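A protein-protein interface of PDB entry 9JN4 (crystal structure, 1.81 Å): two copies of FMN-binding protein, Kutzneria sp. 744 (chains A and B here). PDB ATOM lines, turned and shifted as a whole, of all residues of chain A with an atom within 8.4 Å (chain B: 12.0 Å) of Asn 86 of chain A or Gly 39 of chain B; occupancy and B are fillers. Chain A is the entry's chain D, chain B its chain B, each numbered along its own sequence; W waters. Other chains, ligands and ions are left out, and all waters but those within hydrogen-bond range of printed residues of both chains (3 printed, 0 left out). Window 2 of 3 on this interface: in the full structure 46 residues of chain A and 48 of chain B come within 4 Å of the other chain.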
ATOM      1  N   LEU A  32      11.784 -23.872  34.186  1.00  0.00           N
ATOM      2  CA  LEU A  32      13.074 -24.197  33.526  1.00  0.00           C
ATOM      3  C   LEU A  32      13.148 -25.707  33.343  1.00  0.00           C
ATOM      4  O   LEU A  32      13.134 -26.408  34.381  1.00  0.00           O
ATOM      5  CB  LEU A  32      14.234 -23.647  34.367  1.00  0.00           C
ATOM      6  CG  LEU A  32      15.654 -23.888  33.811  1.00  0.00           C
ATOM      7  CD1 LEU A  32      15.816 -23.390  32.379  1.00  0.00           C
ATOM      8  CD2 LEU A  32      16.704 -23.214  34.691  1.00  0.00           C
ATOM      9  N   ALA A  33      13.289 -26.194  32.084  1.00  0.00           N
ATOM     10  CA  ALA A  33      13.329 -27.639  31.811  1.00  0.00           C
ATOM     11  C   ALA A  33      14.710 -28.010  31.251  1.00  0.00           C
ATOM     12  O   ALA A  33      15.155 -27.343  30.311  1.00  0.00           O
ATOM     13  CB  ALA A  33      12.211 -28.080  30.882  1.00  0.00           C
ATOM     14  N   SER A  34      15.272 -29.116  31.722  1.00  0.00           N
ATOM     15  CA  SER A  34      16.400 -29.764  31.014  1.00  0.00           C
ATOM     16  C   SER A  34      16.264 -31.292  31.008  1.00  0.00           C
ATOM     17  O   SER A  34      15.478 -31.855  31.785  1.00  0.00           O
ATOM     18  CB  SER A  34      17.705 -29.286  31.583  1.00  0.00           C
ATOM     19  OG  SER A  34      17.812 -29.716  32.918  1.00  0.00           O
ATOM     20  N   ASN A  35      16.982 -31.941  30.092  1.00  0.00           N
ATOM     21  CA  ASN A  35      16.843 -33.400  29.891  1.00  0.00           C
ATOM     22  C   ASN A  35      17.235 -34.174  31.150  1.00  0.00           C
ATOM     23  O   ASN A  35      18.225 -33.775  31.874  1.00  0.00           O
ATOM     24  CB  ASN A  35      17.636 -33.911  28.702  1.00  0.00           C
ATOM     25  CG  ASN A  35      17.079 -33.455  27.373  1.00  0.00           C
ATOM     26  OD1 ASN A  35      15.917 -33.054  27.243  1.00  0.00           O
ATOM     27  ND2 ASN A  35      17.925 -33.523  26.355  1.00  0.00           N
ATOM     28  N   HIS A  77      18.699 -30.070  40.398  1.00  0.00           N
ATOM     29  CA  HIS A  77      18.581 -29.602  38.992  1.00  0.00           C
ATOM     30  C   HIS A  77      19.858 -28.805  38.667  1.00  0.00           C
ATOM     31  O   HIS A  77      20.365 -28.867  37.586  1.00  0.00           O
ATOM     32  CB  HIS A  77      17.284 -28.807  38.834  1.00  0.00           C
ATOM     33  CG  HIS A  77      16.928 -28.500  37.405  1.00  0.00           C
ATOM     34  ND1 HIS A  77      15.767 -27.862  37.069  1.00  0.00           N
ATOM     35  CD2 HIS A  77      17.551 -28.774  36.236  1.00  0.00           C
ATOM     36  CE1 HIS A  77      15.660 -27.739  35.738  1.00  0.00           C
ATOM     37  NE2 HIS A  77      16.780 -28.225  35.206  1.00  0.00           N
ATOM     38  N   ALA A  80      22.578 -31.215  37.764  1.00  0.00           N
ATOM     39  CA  ALA A  80      22.215 -32.041  36.619  1.00  0.00           C
ATOM     40  C   ALA A  80      22.409 -31.161  35.378  1.00  0.00           C
ATOM     41  O   ALA A  80      22.729 -31.684  34.319  1.00  0.00           O
ATOM     42  CB  ALA A  80      20.827 -32.575  36.792  1.00  0.00           C
ATOM     43  N   LEU A  81      22.375 -29.844  35.520  1.00  0.00           N
ATOM     44  CA  LEU A  81      22.587 -28.989  34.335  1.00  0.00           C
ATOM     45  C   LEU A  81      23.997 -29.239  33.769  1.00  0.00           C
ATOM     46  O   LEU A  81      24.134 -29.336  32.511  1.00  0.00           O
ATOM     47  CB  LEU A  81      22.314 -27.540  34.700  1.00  0.00           C
ATOM     48  CG  LEU A  81      20.833 -27.225  34.848  1.00  0.00           C
ATOM     49  CD1 LEU A  81      20.630 -25.897  35.596  1.00  0.00           C
ATOM     50  CD2 LEU A  81      20.186 -27.232  33.464  1.00  0.00           C
ATOM     51  N   GLY A  82      24.983 -29.474  34.638  1.00  0.00           N
ATOM     52  CA  GLY A  82      26.381 -29.471  34.200  1.00  0.00           C
ATOM     53  C   GLY A  82      26.628 -28.155  33.498  1.00  0.00           C
ATOM     54  O   GLY A  82      25.869 -27.163  33.858  1.00  0.00           O
ATOM     55  N   GLY A  83      27.468 -28.185  32.445  1.00  0.00           N
ATOM     56  CA  GLY A  83      28.187 -27.012  31.894  1.00  0.00           C
ATOM     57  C   GLY A  83      27.447 -26.318  30.764  1.00  0.00           C
ATOM     58  O   GLY A  83      27.259 -25.081  30.826  1.00  0.00           O
ATOM     59  N   ALA A  84      27.109 -27.039  29.703  1.00  0.00           N
ATOM     60  CA  ALA A  84      26.531 -26.436  28.477  1.00  0.00           C
ATOM     61  C   ALA A  84      25.184 -27.087  28.175  1.00  0.00           C
ATOM     62  O   ALA A  84      25.007 -27.596  27.060  1.00  0.00           O
ATOM     63  CB  ALA A  84      27.495 -26.573  27.335  1.00  0.00           C
ATOM     64  N   ALA A  85      24.274 -27.062  29.152  1.00  0.00           N
ATOM     65  CA  ALA A  85      22.947 -27.709  29.046  1.00  0.00           C
ATOM     66  C   ALA A  85      22.102 -26.905  28.065  1.00  0.00           C
ATOM     67  O   ALA A  85      22.034 -25.660  28.216  1.00  0.00           O
ATOM     68  CB  ALA A  85      22.254 -27.808  30.375  1.00  0.00           C
ATOM     69  N   ASN A  86      21.503 -27.606  27.103  1.00  0.00           N
ATOM     70  CA  ASN A  86      20.447 -27.045  26.229  1.00  0.00           C
ATOM     71  C   ASN A  86      19.138 -27.065  27.011  1.00  0.00           C
ATOM     72  O   ASN A  86      18.720 -28.164  27.435  1.00  0.00           O
ATOM     73  CB  ASN A  86      20.323 -27.802  24.935  1.00  0.00           C
ATOM     74  CG  ASN A  86      21.606 -27.756  24.150  1.00  0.00           C
ATOM     75  OD1 ASN A  86      22.224 -26.701  24.057  1.00  0.00           O
ATOM     76  ND2 ASN A  86      21.998 -28.895  23.616  1.00  0.00           N
ATOM     77  N   VAL A  87      18.582 -25.884  27.247  1.00  0.00           N
ATOM     78  CA  VAL A  87      17.401 -25.774  28.137  1.00  0.00           C
ATOM     79  C   VAL A  87      16.249 -25.083  27.420  1.00  0.00           C
ATOM     80  O   VAL A  87      16.447 -24.425  26.400  1.00  0.00           O
ATOM     81  CB  VAL A  87      17.744 -25.070  29.455  1.00  0.00           C
ATOM     82  CG1 VAL A  87      18.891 -25.771  30.135  1.00  0.00           C
ATOM     83  CG2 VAL A  87      18.020 -23.595  29.285  1.00  0.00           C
ATOM     84  N   VAL A  88      15.047 -25.285  27.950  1.00  0.00           N
ATOM     85  CA  VAL A  88      13.859 -24.473  27.585  1.00  0.00           C
ATOM     86  C   VAL A  88      13.348 -23.806  28.854  1.00  0.00           C
ATOM     87  O   VAL A  88      13.361 -24.425  29.926  1.00  0.00           O
ATOM     88  CB  VAL A  88      12.753 -25.283  26.875  1.00  0.00           C
ATOM     89  CG1 VAL A  88      12.423 -26.561  27.629  1.00  0.00           C
ATOM     90  CG2 VAL A  88      11.519 -24.441  26.675  1.00  0.00           C
ATOM     91  N   ALA A  89      12.989 -22.542  28.741  1.00  0.00           N
ATOM     92  CA  ALA A  89      12.330 -21.793  29.825  1.00  0.00           C
ATOM     93  C   ALA A  89      10.947 -21.423  29.297  1.00  0.00           C
ATOM     94  O   ALA A  89      10.881 -20.802  28.201  1.00  0.00           O
ATOM     95  CB  ALA A  89      13.130 -20.596  30.232  1.00  0.00           C
ATOM     96  N   VAL A 119      11.449 -20.225  25.410  1.00  0.00           N
ATOM     97  CA  VAL A 119      12.817 -19.786  24.985  1.00  0.00           C
ATOM     98  C   VAL A 119      13.765 -20.957  25.158  1.00  0.00           C
ATOM     99  O   VAL A 119      13.671 -21.684  26.129  1.00  0.00           O
ATOM    100  CB  VAL A 119      13.376 -18.553  25.722  1.00  0.00           C
ATOM    101  CG1 VAL A 119      12.634 -17.278  25.382  1.00  0.00           C
ATOM    102  CG2 VAL A 119      13.405 -18.767  27.214  1.00  0.00           C
ATOM    103  N   ARG A 120      14.632 -21.151  24.180  1.00  0.00           N
ATOM    104  CA  ARG A 120      15.627 -22.237  24.215  1.00  0.00           C
ATOM    105  C   ARG A 120      17.012 -21.633  23.943  1.00  0.00           C
ATOM    106  O   ARG A 120      17.142 -20.658  23.079  1.00  0.00           O
ATOM    107  CB  ARG A 120      15.265 -23.332  23.208  1.00  0.00           C
ATOM    108  CG  ARG A 120      13.958 -24.046  23.525  1.00  0.00           C
ATOM    109  CD  ARG A 120      13.613 -25.020  22.390  1.00  0.00           C
ATOM    110  NE  ARG A 120      12.714 -26.021  22.919  1.00  0.00           N
ATOM    111  CZ  ARG A 120      11.419 -25.848  23.208  1.00  0.00           C
ATOM    112  NH1 ARG A 120      10.769 -24.697  22.995  1.00  0.00           N
ATOM    113  NH2 ARG A 120      10.780 -26.900  23.681  1.00  0.00           N
ATOM    114  N   GLY A 121      17.992 -22.210  24.637  1.00  0.00           N
ATOM    115  CA  GLY A 121      19.413 -22.019  24.347  1.00  0.00           C
ATOM    116  C   GLY A 121      20.275 -22.617  25.432  1.00  0.00           C
ATOM    117  O   GLY A 121      19.769 -23.495  26.200  1.00  0.00           O
ATOM    118  N   GLU A 122      21.536 -22.179  25.491  1.00  0.00           N
ATOM    119  CA  GLU A 122      22.543 -22.761  26.394  1.00  0.00           C
ATOM    120  C   GLU A 122      22.496 -22.048  27.725  1.00  0.00           C
ATOM    121  O   GLU A 122      22.556 -20.819  27.748  1.00  0.00           O
ATOM    122  CB  GLU A 122      23.966 -22.610  25.884  1.00  0.00           C
ATOM    123  CG  GLU A 122      24.216 -23.482  24.668  1.00  0.00           C
ATOM    124  CD  GLU A 122      25.672 -23.651  24.261  1.00  0.00           C
ATOM    125  OE1 GLU A 122      26.561 -23.435  25.129  1.00  0.00           O
ATOM    126  OE2 GLU A 122      25.906 -23.974  23.066  1.00  0.00           O
ATOM    127  N   LEU A 123      22.363 -22.814  28.790  1.00  0.00           N
ATOM    128  CA  LEU A 123      22.398 -22.244  30.130  1.00  0.00           C
ATOM    129  C   LEU A 123      23.854 -22.230  30.608  1.00  0.00           C
ATOM    130  O   LEU A 123      24.497 -23.315  30.682  1.00  0.00           O
ATOM    131  CB  LEU A 123      21.495 -23.045  31.054  1.00  0.00           C
ATOM    132  CG  LEU A 123      21.419 -22.392  32.439  1.00  0.00           C
ATOM    133  CD1 LEU A 123      20.045 -22.573  33.052  1.00  0.00           C
ATOM    134  CD2 LEU A 123      22.462 -22.955  33.380  1.00  0.00           C
ATOM    135  N   ARG A 124      24.342 -21.056  30.986  1.00  0.00           N
ATOM    136  CA  ARG A 124      25.679 -20.922  31.611  1.00  0.00           C
ATOM    137  C   ARG A 124      25.491 -20.572  33.082  1.00  0.00           C
ATOM    138  O   ARG A 124      24.762 -19.597  33.390  1.00  0.00           O
ATOM    139  CB  ARG A 124      26.537 -19.874  30.926  1.00  0.00           C
ATOM    140  CG  ARG A 124      27.924 -19.828  31.553  1.00  0.00           C
ATOM    141  CD  ARG A 124      28.820 -18.742  31.006  1.00  0.00           C
ATOM    142  NE  ARG A 124      28.345 -17.372  31.214  1.00  0.00           N
ATOM    143  CZ  ARG A 124      28.356 -16.710  32.378  1.00  0.00           C
ATOM    144  NH1 ARG A 124      28.744 -17.290  33.504  1.00  0.00           N
ATOM    145  NH2 ARG A 124      27.956 -15.455  32.408  1.00  0.00           N
ATOM    146  N   LEU A 172      20.991 -17.184  30.171  1.00  0.00           N
ATOM    147  CA  LEU A 172      20.402 -18.013  29.097  1.00  0.00           C
ATOM    148  C   LEU A 172      20.390 -17.136  27.834  1.00  0.00           C
ATOM    149  O   LEU A 172      19.568 -16.214  27.705  1.00  0.00           O
ATOM    150  CB  LEU A 172      19.017 -18.525  29.510  1.00  0.00           C
ATOM    151  CG  LEU A 172      18.324 -19.416  28.477  1.00  0.00           C
ATOM    152  CD1 LEU A 172      19.197 -20.619  28.135  1.00  0.00           C
ATOM    153  CD2 LEU A 172      16.977 -19.874  28.992  1.00  0.00           C
ATOM    154  N   ARG A 173      21.356 -17.396  26.979  1.00  0.00           N
ATOM    155  CA  ARG A 173      21.474 -16.845  25.612  1.00  0.00           C
ATOM    156  C   ARG A 173      20.329 -17.456  24.804  1.00  0.00           C
ATOM    157  O   ARG A 173      20.360 -18.624  24.641  1.00  0.00           O
ATOM    158  CB  ARG A 173      22.871 -17.247  25.095  1.00  0.00           C
ATOM    159  CG  ARG A 173      23.252 -16.692  23.733  1.00  0.00           C
ATOM    160  CD  ARG A 173      22.777 -15.278  23.466  1.00  0.00           C
ATOM    161  NE  ARG A 173      23.573 -14.580  22.443  1.00  0.00           N
ATOM    162  CZ  ARG A 173      23.549 -14.811  21.121  1.00  0.00           C
ATOM    163  NH1 ARG A 173      24.307 -14.088  20.317  1.00  0.00           N
ATOM    164  NH2 ARG A 173      22.783 -15.757  20.600  1.00  0.00           N
ATOM    165  N   ALA A 175      18.559 -18.638  21.773  1.00  0.00           N
ATOM    166  CA  ALA A 175      18.838 -19.074  20.377  1.00  0.00           C
ATOM    167  C   ALA A 175      17.518 -19.145  19.604  1.00  0.00           C
ATOM    168  O   ALA A 175      17.495 -18.874  18.415  1.00  0.00           O
ATOM    169  CB  ALA A 175      19.500 -20.431  20.399  1.00  0.00           C
ATOM    170  N   ALA B  33       6.346 -32.483  29.515  1.00  0.00           N
ATOM    171  CA  ALA B  33       7.762 -32.378  29.117  1.00  0.00           C
ATOM    172  C   ALA B  33       8.320 -33.784  28.884  1.00  0.00           C
ATOM    173  O   ALA B  33       8.136 -34.664  29.731  1.00  0.00           O
ATOM    174  CB  ALA B  33       8.587 -31.615  30.147  1.00  0.00           C
ATOM    175  N   SER B  34       9.062 -33.946  27.804  1.00  0.00           N
ATOM    176  CA  SER B  34       9.902 -35.141  27.574  1.00  0.00           C
ATOM    177  C   SER B  34      11.229 -34.676  26.983  1.00  0.00           C
ATOM    178  O   SER B  34      11.302 -33.549  26.477  1.00  0.00           O
ATOM    179  CB  SER B  34       9.208 -36.104  26.672  1.00  0.00           C
ATOM    180  OG  SER B  34       8.992 -35.502  25.407  1.00  0.00           O
ATOM    181  N   ASN B  35      12.225 -35.551  27.049  1.00  0.00           N
ATOM    182  CA  ASN B  35      13.612 -35.268  26.644  1.00  0.00           C
ATOM    183  C   ASN B  35      13.626 -34.918  25.155  1.00  0.00           C
ATOM    184  O   ASN B  35      12.931 -35.585  24.357  1.00  0.00           O
ATOM    185  CB  ASN B  35      14.548 -36.433  26.924  1.00  0.00           C
ATOM    186  CG  ASN B  35      14.851 -36.613  28.379  1.00  0.00           C
ATOM    187  OD1 ASN B  35      14.552 -35.726  29.191  1.00  0.00           O
ATOM    188  ND2 ASN B  35      15.495 -37.735  28.701  1.00  0.00           N
ATOM    189  N   GLY B  36      14.458 -33.947  24.806  1.00  0.00           N
ATOM    190  CA  GLY B  36      14.848 -33.687  23.419  1.00  0.00           C
ATOM    191  C   GLY B  36      15.852 -34.729  22.949  1.00  0.00           C
ATOM    192  O   GLY B  36      16.623 -35.221  23.771  1.00  0.00           O
ATOM    193  N   ALA B  37      15.837 -35.041  21.657  1.00  0.00           N
ATOM    194  CA  ALA B  37      16.785 -36.000  21.038  1.00  0.00           C
ATOM    195  C   ALA B  37      18.158 -35.330  20.959  1.00  0.00           C
ATOM    196  O   ALA B  37      18.193 -34.092  20.656  1.00  0.00           O
ATOM    197  CB  ALA B  37      16.287 -36.412  19.681  1.00  0.00           C
ATOM    198  N   GLY B  38      19.206 -36.107  21.278  1.00  0.00           N
ATOM    199  CA  GLY B  38      20.619 -35.794  21.015  1.00  0.00           C
ATOM    200  C   GLY B  38      21.022 -34.497  21.689  1.00  0.00           C
ATOM    201  O   GLY B  38      21.553 -33.601  20.999  1.00  0.00           O
ATOM    202  N   GLY B  39      20.710 -34.378  22.980  1.00  0.00           N
ATOM    203  CA  GLY B  39      21.098 -33.220  23.805  1.00  0.00           C
ATOM    204  C   GLY B  39      20.255 -31.968  23.577  1.00  0.00           C
ATOM    205  O   GLY B  39      20.589 -30.973  24.255  1.00  0.00           O
ATOM    206  N   ALA B  40      19.220 -31.979  22.711  1.00  0.00           N
ATOM    207  CA  ALA B  40      18.328 -30.807  22.478  1.00  0.00           C
ATOM    208  C   ALA B  40      17.542 -30.576  23.760  1.00  0.00           C
ATOM    209  O   ALA B  40      17.511 -31.509  24.582  1.00  0.00           O
ATOM    210  CB  ALA B  40      17.381 -30.950  21.309  1.00  0.00           C
ATOM    211  N   ALA B  41      16.967 -29.384  23.923  1.00  0.00           N
ATOM    212  CA  ALA B  41      16.137 -29.057  25.109  1.00  0.00           C
ATOM    213  C   ALA B  41      14.871 -29.910  25.053  1.00  0.00           C
ATOM    214  O   ALA B  41      14.460 -30.331  23.953  1.00  0.00           O
ATOM    215  CB  ALA B  41      15.817 -27.579  25.192  1.00  0.00           C
ATOM    216  N   PRO B  42      14.251 -30.209  26.220  1.00  0.00           N
ATOM    217  CA  PRO B  42      12.969 -30.912  26.266  1.00  0.00           C
ATOM    218  C   PRO B  42      11.896 -30.306  25.341  1.00  0.00           C
ATOM    219  O   PRO B  42      11.886 -29.103  25.161  1.00  0.00           O
ATOM    220  CB  PRO B  42      12.566 -30.780  27.743  1.00  0.00           C
ATOM    221  CG  PRO B  42      13.909 -30.744  28.470  1.00  0.00           C
ATOM    222  CD  PRO B  42      14.773 -29.919  27.575  1.00  0.00           C
ATOM    223  N   HIS B  43      11.016 -31.164  24.808  1.00  0.00           N
ATOM    224  CA  HIS B  43       9.731 -30.797  24.168  1.00  0.00           C
ATOM    225  C   HIS B  43       8.763 -30.429  25.290  1.00  0.00           C
ATOM    226  O   HIS B  43       8.794 -31.121  26.314  1.00  0.00           O
ATOM    227  CB  HIS B  43       9.092 -31.956  23.379  1.00  0.00           C
ATOM    228  CG  HIS B  43       9.969 -32.528  22.338  1.00  0.00           C
ATOM    229  ND1 HIS B  43       9.865 -32.154  21.028  1.00  0.00           N
ATOM    230  CD2 HIS B  43      10.898 -33.495  22.400  1.00  0.00           C
ATOM    231  CE1 HIS B  43      10.734 -32.847  20.324  1.00  0.00           C
ATOM    232  NE2 HIS B  43      11.380 -33.659  21.137  1.00  0.00           N
ATOM    233  N   ILE B  44       8.073 -29.303  25.162  1.00  0.00           N
ATOM    234  CA  ILE B  44       7.062 -28.856  26.163  1.00  0.00           C
ATOM    235  C   ILE B  44       5.757 -28.567  25.421  1.00  0.00           C
ATOM    236  O   ILE B  44       5.763 -27.753  24.431  1.00  0.00           O
ATOM    237  CB  ILE B  44       7.551 -27.583  26.868  1.00  0.00           C
ATOM    238  CG1 ILE B  44       8.950 -27.704  27.481  1.00  0.00           C
ATOM    239  CG2 ILE B  44       6.491 -27.171  27.876  1.00  0.00           C
ATOM    240  CD1 ILE B  44       8.902 -28.373  28.825  1.00  0.00           C
HETATM  241  O   HOH W   1      22.390 -30.490  26.743  1.00  0.00           O
HETATM  242  O   HOH W   2      13.572 -28.661  22.241  1.00  0.00           O
HETATM  243  O   HOH W   3       8.267 -27.838  22.488  1.00  0.00           O
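N of Gly 36 of chain B sits at hydrogen-bond distance from OD1 of Asn 35 of chain A, 3.0 Å away.
O of Gly 39 of chain B sits at hydrogen-bond distance from ND2 of Asn 86 of chain A, 2.6 Å away.
The backbone carbonyl oxygen (O) of Ala 40 of chain B lies within hydrogen-bond range of the side-chain amide nitrogen (ND2) of Asn 35 of chain A.
NH2 of Arg 120 of chain A is in hydrogen-bond range of O of Pro 42 of chain B.
OD1 of Asn 35 of chain A sits close to N of Pro 42 of chain B, 3.5 Å away.
The backbone NH (N) of Ala 33 of chain A lies within hydrogen-bond range of the backbone carbonyl oxygen (O) of Val 88 of chain A (2.8 Å).
The side-chain hydroxyl of Ser 34 of chain A sits at hydrogen-bond distance from a ring nitrogen (NE2) of His 77 of chain A (2.9 Å).
N of Val 87 of chain A lies within hydrogen-bond range of O of Gly 121 of chain A (2.9 Å).
The backbone NH (N) of Ala 175 of chain A is in hydrogen-bond range of the backbone carbonyl oxygen (O) of Arg 120 of chain A (2.8 Å).
Among the printed residues, merely in contact across the chains: Ala 33 of chain A with Pro 42 of chain B (3.8 Å), Ala 33 of chain A with Ile 44 of chain B (3.9 Å), Ser 34 of chain A with Pro 42 of chain B (3.5 Å), Asn 35 of chain A with Asn 35 of chain B (3.3 Å), Asn 35 of chain A with Gly 39 of chain B (3.9 Å), Asn 35 of chain A with Ala 41 of chain B (3.97 Å), Asn 86 of chain A with Ala 41 of chain B (3.6 Å), Val 87 of chain A with Ala 41 of chain B (3.4 Å), Val 88 of chain A with Ala 41 of chain B (3.7 Å), Val 88 of chain A with Pro 42 of chain B (3.6 Å), Val 88 of chain A with Ile 44 of chain B (3.7 Å) and Arg 120 of chain A with Ile 44 of chain B (3.9 Å).
Asn 86 of chain A touches just these residues of chain B: Gly 39 and Ala 41.
Gly 39 of chain B touches just these residues of chain A: Asn 35 (3.9 Å) and Asn 86 (2.6 Å).
Of chain B, only Pro 42 (3.8 Å) and Ile 44 (3.9 Å) come within 4 Å of Ala 33 of chain A.
Of chain B, only Pro 42 comes within 4 Å of Ser 34 of chain A.
Of chain B, only Asn 35 (3.3 Å), Gly 36 (3.0 Å), Gly 39 (3.9 Å), Ala 40 (2.7 Å), Ala 41 (3.97 Å) and Pro 42 (3.3 Å) come within 4 Å of Asn 35 of chain A.
No residue of chain B comes within 4 Å of Ala 84 of chain A.
No residue of chain B comes within 4 Å of Ala 85 of chain A.
Of chain B, only Ala 41 (3.4 Å) comes within 4 Å of Val 87 of chain A.
No residue of chain B comes within 4 Å of Gly 121 of chain A.
No residue of chain B comes within 4 Å of Glu 122 of chain A.
No residue of chain A comes within 4 Å of Gly 38 of chain B.
Ala 40 of chain B touches just one residue of chain A: Asn 35 (2.7 Å).
Of the printed residues of chain A, Ile 44 of chain B touches Ala 33 (3.9 Å), Val 88 (3.7 Å) and Arg 120 (3.9 Å).
Printed residues of chain A within 4 Å of Asn 35 of chain B: Asn 35 (3.3 Å).
Of the printed residues of chain B, Val 88 of chain A touches Ala 41 (3.7 Å), Pro 42 (3.6 Å) and Ile 44 (3.7 Å).
Printed residues of chain B within 4 Å of Arg 120 of chain A: Pro 42 and Ile 44.
Printed residues of chain A within 4 Å of Pro 42 of chain B: Ala 33 (3.8 Å), Ser 34 (3.5 Å), Asn 35 (3.3 Å), Val 88 (3.6 Å) and Arg 120 (2.9 Å).
The nearest residue of chain A that does not touch Gly 39 of chain B is Ala 85 of chain A (5.8 Å).
The nearest printed residue of chain B that does not touch Arg 120 of chain A is His 43 of chain B (4.1 Å).
Printed residues of chain A that touch a printed residue of chain B: Ala 33, Ser 34, Asn 35, Asn 86, Val 87, Val 88 and Arg 120.
Hydrophobic or aromatic side chains of chain A within 4 Å of the printed part of chain B: Ala 33 and Val 88.
Hydrophobic or aromatic side chains of chain B that line the printed part of chain A: Ala 41, Pro 42 and Ile 44.
Among the printed residues, 17 pairs touch across the chains.
Asn 35 of chain B touches its own counterpart, Asn 35 of chain A.
Of the 17 pairs that touch across the chains among the printed residues, 1 has its exchanged pair printed and touching as well.
Water W2 lies within hydrogen-bond range of the backbone carbonyl oxygen (O) of Ala 41 of chain B (2.6 Å), the guanidinium group (NE) of Arg 120 of chain A (2.9 Å) and the backbone carbonyl oxygen (O) of Pro 42 of chain B (3.4 Å).
Water W3 lies within hydrogen-bond range of NH2 of Arg 120 of chain A (2.9 Å) and N of Ile 44 of chain B (3.1 Å).
Water W1 bridges N of Asn 86 of chain A (3.0 Å) and O of Gly 39 of chain B (3.1 Å).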
